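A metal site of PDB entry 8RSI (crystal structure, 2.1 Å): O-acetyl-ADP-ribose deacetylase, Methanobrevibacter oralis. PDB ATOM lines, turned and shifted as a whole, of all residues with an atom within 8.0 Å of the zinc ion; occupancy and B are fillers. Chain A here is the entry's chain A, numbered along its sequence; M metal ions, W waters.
The backbone carbonyl oxygen of His 114 lies close to the side-chain amide oxygen of Asn 119.
The guanidinium group of Arg 38 is in hydrogen-bond range of the backbone carbonyl oxygen of His 114, 3.0 Å away.
The side-chain sulfur (SG) of Cys 116 lies close to the backbone NH (N) of Asn 119, at 3.4 Å.
The side-chain sulfur (SG) of Cys 109 lies close to the side-chain amide nitrogen (ND2) of Asn 119, 3.4 Å away.
N of Ile 111 lies close to SG of Cys 109.
Of the 17 residues printed, 3 come within 4 Å of the zinc ion.
The nearest printed residue that does not touch the zinc ion is Asn 119 (4.4 Å).
A ring nitrogen (ND1) of His 114 is bound to the zinc ion (2.1 Å).
SG of Cys 116 is bound to the zinc ion, 2.3 Å away.
SG of Cys 109 is bound to the zinc ion.
The zinc ion has three donor atoms within binding distance.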
ATOM      1  N   ARG A  38     -30.668  10.929  16.989  1.00  0.00           N
ATOM      2  CA  ARG A  38     -29.814  11.554  17.980  1.00  0.00           C
ATOM      3  C   ARG A  38     -29.893  10.797  19.304  1.00  0.00           C
ATOM      4  O   ARG A  38     -28.869  10.401  19.859  1.00  0.00           O
ATOM      5  CB  ARG A  38     -30.180  13.028  18.080  1.00  0.00           C
ATOM      6  CG  ARG A  38     -29.451  13.761  19.195  1.00  0.00           C
ATOM      7  CD  ARG A  38     -29.585  15.265  19.114  1.00  0.00           C
ATOM      8  NE  ARG A  38     -29.054  15.855  20.328  1.00  0.00           N
ATOM      9  CZ  ARG A  38     -29.373  17.064  20.772  1.00  0.00           C
ATOM     10  NH1 ARG A  38     -30.249  17.806  20.104  1.00  0.00           N
ATOM     11  NH2 ARG A  38     -28.834  17.528  21.882  1.00  0.00           N
ATOM     12  N   ASN A  42     -26.957   9.069  21.175  1.00  0.00           N
ATOM     13  CA  ASN A  42     -26.609   9.520  22.504  1.00  0.00           C
ATOM     14  C   ASN A  42     -26.439   8.326  23.434  1.00  0.00           C
ATOM     15  O   ASN A  42     -25.505   8.298  24.231  1.00  0.00           O
ATOM     16  CB  ASN A  42     -27.671  10.460  23.094  1.00  0.00           C
ATOM     17  CG  ASN A  42     -27.766  11.829  22.436  1.00  0.00           C
ATOM     18  OD1 ASN A  42     -28.744  12.547  22.622  1.00  0.00           O
ATOM     19  ND2 ASN A  42     -26.778  12.203  21.656  1.00  0.00           N
ATOM     20  N   ASN A 103     -17.182  15.704  30.299  1.00  0.00           N
ATOM     21  CA  ASN A 103     -17.126  15.097  31.624  1.00  0.00           C
ATOM     22  C   ASN A 103     -15.954  14.109  31.745  1.00  0.00           C
ATOM     23  O   ASN A 103     -15.299  13.746  30.755  1.00  0.00           O
ATOM     24  CB  ASN A 103     -18.427  14.379  31.973  1.00  0.00           C
ATOM     25  CG  ASN A 103     -18.797  13.292  30.982  1.00  0.00           C
ATOM     26  OD1 ASN A 103     -18.123  12.266  30.855  1.00  0.00           O
ATOM     27  ND2 ASN A 103     -19.868  13.517  30.250  1.00  0.00           N
ATOM     28  N   GLY A 108     -18.919  11.631  26.317  1.00  0.00           N
ATOM     29  CA  GLY A 108     -20.016  12.493  25.913  1.00  0.00           C
ATOM     30  C   GLY A 108     -21.202  12.322  26.845  1.00  0.00           C
ATOM     31  O   GLY A 108     -21.018  11.904  27.967  1.00  0.00           O
ATOM     32  N   CYS A 109     -22.407  12.575  26.312  1.00  0.00           N
ATOM     33  CA  CYS A 109     -23.638  12.652  27.086  1.00  0.00           C
ATOM     34  C   CYS A 109     -24.619  11.551  26.682  1.00  0.00           C
ATOM     35  O   CYS A 109     -25.026  11.431  25.536  1.00  0.00           O
ATOM     36  CB  CYS A 109     -24.264  14.034  26.885  1.00  0.00           C
ATOM     37  SG  CYS A 109     -25.915  14.158  27.618  1.00  0.00           S
ATOM     38  N   PHE A 110     -25.002  10.728  27.641  1.00  0.00           N
ATOM     39  CA  PHE A 110     -25.810   9.542  27.379  1.00  0.00           C
ATOM     40  C   PHE A 110     -27.307   9.840  27.515  1.00  0.00           C
ATOM     41  O   PHE A 110     -28.125   8.960  27.251  1.00  0.00           O
ATOM     42  CB  PHE A 110     -25.368   8.411  28.286  1.00  0.00           C
ATOM     43  CG  PHE A 110     -24.129   7.717  27.779  1.00  0.00           C
ATOM     44  CD1 PHE A 110     -24.228   6.770  26.772  1.00  0.00           C
ATOM     45  CD2 PHE A 110     -22.885   8.039  28.279  1.00  0.00           C
ATOM     46  CE1 PHE A 110     -23.087   6.157  26.272  1.00  0.00           C
ATOM     47  CE2 PHE A 110     -21.746   7.407  27.801  1.00  0.00           C
ATOM     48  CZ  PHE A 110     -21.845   6.491  26.764  1.00  0.00           C
ATOM     49  N   ILE A 111     -27.653  11.089  27.861  1.00  0.00           N
ATOM     50  CA  ILE A 111     -29.042  11.475  28.029  1.00  0.00           C
ATOM     51  C   ILE A 111     -29.631  11.948  26.702  1.00  0.00           C
ATOM     52  O   ILE A 111     -29.160  12.946  26.158  1.00  0.00           O
ATOM     53  CB  ILE A 111     -29.163  12.576  29.089  1.00  0.00           C
ATOM     54  CG1 ILE A 111     -28.682  12.072  30.451  1.00  0.00           C
ATOM     55  CG2 ILE A 111     -30.592  13.091  29.115  1.00  0.00           C
ATOM     56  CD1 ILE A 111     -28.570  13.145  31.506  1.00  0.00           C
ATOM     57  N   PRO A 112     -30.673  11.276  26.175  1.00  0.00           N
ATOM     58  CA  PRO A 112     -31.212  11.589  24.857  1.00  0.00           C
ATOM     59  C   PRO A 112     -31.716  13.024  24.770  1.00  0.00           C
ATOM     60  O   PRO A 112     -32.357  13.497  25.688  1.00  0.00           O
ATOM     61  CB  PRO A 112     -32.364  10.605  24.614  1.00  0.00           C
ATOM     62  CG  PRO A 112     -32.303   9.602  25.740  1.00  0.00           C
ATOM     63  CD  PRO A 112     -31.351  10.126  26.797  1.00  0.00           C
ATOM     64  N   MET A 113     -31.295  13.743  23.729  1.00  0.00           N
ATOM     65  CA  MET A 113     -31.841  15.056  23.398  1.00  0.00           C
ATOM     66  C   MET A 113     -31.312  16.141  24.333  1.00  0.00           C
ATOM     67  O   MET A 113     -31.694  17.290  24.206  1.00  0.00           O
ATOM     68  CB  MET A 113     -33.374  15.076  23.501  1.00  0.00           C
ATOM     69  CG  MET A 113     -34.085  14.158  22.530  1.00  0.00           C
ATOM     70  SD  MET A 113     -33.706  14.587  20.817  1.00  0.00           S
ATOM     71  CE  MET A 113     -32.384  13.427  20.523  1.00  0.00           C
ATOM     72  N   HIS A 114     -30.420  15.791  25.257  1.00  0.00           N
ATOM     73  CA  HIS A 114     -29.979  16.753  26.265  1.00  0.00           C
ATOM     74  C   HIS A 114     -29.207  17.873  25.589  1.00  0.00           C
ATOM     75  O   HIS A 114     -28.293  17.578  24.831  1.00  0.00           O
ATOM     76  CB  HIS A 114     -29.142  16.053  27.331  1.00  0.00           C
ATOM     77  CG  HIS A 114     -28.907  16.931  28.511  1.00  0.00           C
ATOM     78  ND1 HIS A 114     -27.655  17.218  29.022  1.00  0.00           N
ATOM     79  CD2 HIS A 114     -29.798  17.593  29.258  1.00  0.00           C
ATOM     80  CE1 HIS A 114     -27.795  18.045  30.038  1.00  0.00           C
ATOM     81  NE2 HIS A 114     -29.090  18.295  30.188  1.00  0.00           N
ATOM     82  N   ASN A 115     -29.478  19.136  25.933  1.00  0.00           N
ATOM     83  CA  ASN A 115     -28.850  20.202  25.135  1.00  0.00           C
ATOM     84  C   ASN A 115     -27.672  20.807  25.900  1.00  0.00           C
ATOM     85  O   ASN A 115     -27.468  22.020  25.935  1.00  0.00           O
ATOM     86  CB  ASN A 115     -29.884  21.090  24.421  1.00  0.00           C
ATOM     87  CG  ASN A 115     -30.473  20.405  23.187  1.00  0.00           C
ATOM     88  OD1 ASN A 115     -29.926  20.457  22.094  1.00  0.00           O
ATOM     89  ND2 ASN A 115     -31.614  19.744  23.341  1.00  0.00           N
ATOM     90  N   CYS A 116     -26.798  19.930  26.392  1.00  0.00           N
ATOM     91  CA  CYS A 116     -25.449  20.356  26.737  1.00  0.00           C
ATOM     92  C   CYS A 116     -24.565  20.300  25.475  1.00  0.00           C
ATOM     93  O   CYS A 116     -24.797  19.528  24.551  1.00  0.00           O
ATOM     94  CB  CYS A 116     -24.913  19.498  27.888  1.00  0.00           C
ATOM     95  SG  CYS A 116     -24.571  17.772  27.406  1.00  0.00           S
ATOM     96  N   ILE A 117     -23.517  21.111  25.445  1.00  0.00           N
ATOM     97  CA  ILE A 117     -22.627  21.209  24.321  1.00  0.00           C
ATOM     98  C   ILE A 117     -22.016  19.836  24.036  1.00  0.00           C
ATOM     99  O   ILE A 117     -21.785  19.527  22.870  1.00  0.00           O
ATOM    100  CB  ILE A 117     -21.529  22.268  24.561  1.00  0.00           C
ATOM    101  CG1 ILE A 117     -20.972  22.826  23.260  1.00  0.00           C
ATOM    102  CG2 ILE A 117     -20.400  21.746  25.427  1.00  0.00           C
ATOM    103  CD1 ILE A 117     -22.068  23.235  22.313  1.00  0.00           C
ATOM    104  N   ASP A 118     -21.747  19.026  25.081  1.00  0.00           N
ATOM    105  CA  ASP A 118     -21.124  17.717  24.907  1.00  0.00           C
ATOM    106  C   ASP A 118     -22.029  16.880  24.027  1.00  0.00           C
ATOM    107  O   ASP A 118     -21.607  16.339  23.001  1.00  0.00           O
ATOM    108  CB  ASP A 118     -20.842  17.055  26.262  1.00  0.00           C
ATOM    109  CG  ASP A 118     -19.872  15.884  26.258  1.00  0.00           C
ATOM    110  OD1 ASP A 118     -19.140  15.694  25.256  1.00  0.00           O
ATOM    111  OD2 ASP A 118     -19.876  15.106  27.262  1.00  0.00           O
ATOM    112  N   ASN A 119     -23.308  16.863  24.376  1.00  0.00           N
ATOM    113  CA  ASN A 119     -24.281  16.131  23.589  1.00  0.00           C
ATOM    114  C   ASN A 119     -24.325  16.631  22.138  1.00  0.00           C
ATOM    115  O   ASN A 119     -24.316  15.827  21.202  1.00  0.00           O
ATOM    116  CB  ASN A 119     -25.665  16.220  24.213  1.00  0.00           C
ATOM    117  CG  ASN A 119     -26.625  15.233  23.631  1.00  0.00           C
ATOM    118  OD1 ASN A 119     -27.010  15.363  22.469  1.00  0.00           O
ATOM    119  ND2 ASN A 119     -27.013  14.234  24.432  1.00  0.00           N
ATOM    120  N   ILE A 120     -24.394  17.944  21.971  1.00  0.00           N
ATOM    121  CA  ILE A 120     -24.577  18.548  20.678  1.00  0.00           C
ATOM    122  C   ILE A 120     -23.385  18.211  19.763  1.00  0.00           C
ATOM    123  O   ILE A 120     -23.586  17.944  18.576  1.00  0.00           O
ATOM    124  CB  ILE A 120     -24.711  20.063  20.895  1.00  0.00           C
ATOM    125  CG1 ILE A 120     -26.039  20.412  21.583  1.00  0.00           C
ATOM    126  CG2 ILE A 120     -24.485  20.805  19.572  1.00  0.00           C
ATOM    127  CD1 ILE A 120     -26.118  21.870  21.988  1.00  0.00           C
ATOM    128  N   VAL A 212     -24.323  23.261  33.236  1.00  0.00           N
ATOM    129  CA  VAL A 212     -24.454  22.029  33.999  1.00  0.00           C
ATOM    130  C   VAL A 212     -23.547  22.082  35.222  1.00  0.00           C
ATOM    131  O   VAL A 212     -23.959  21.684  36.290  1.00  0.00           O
ATOM    132  CB  VAL A 212     -24.066  20.776  33.158  1.00  0.00           C
ATOM    133  CG1 VAL A 212     -24.268  19.487  33.948  1.00  0.00           C
ATOM    134  CG2 VAL A 212     -24.805  20.696  31.838  1.00  0.00           C
HETATM  135 ZN    ZN M   1     -25.811  16.256  28.653  1.00  0.00          ZN
HETATM  136  O   HOH W   1     -24.876  16.043  31.351  1.00  0.00           O
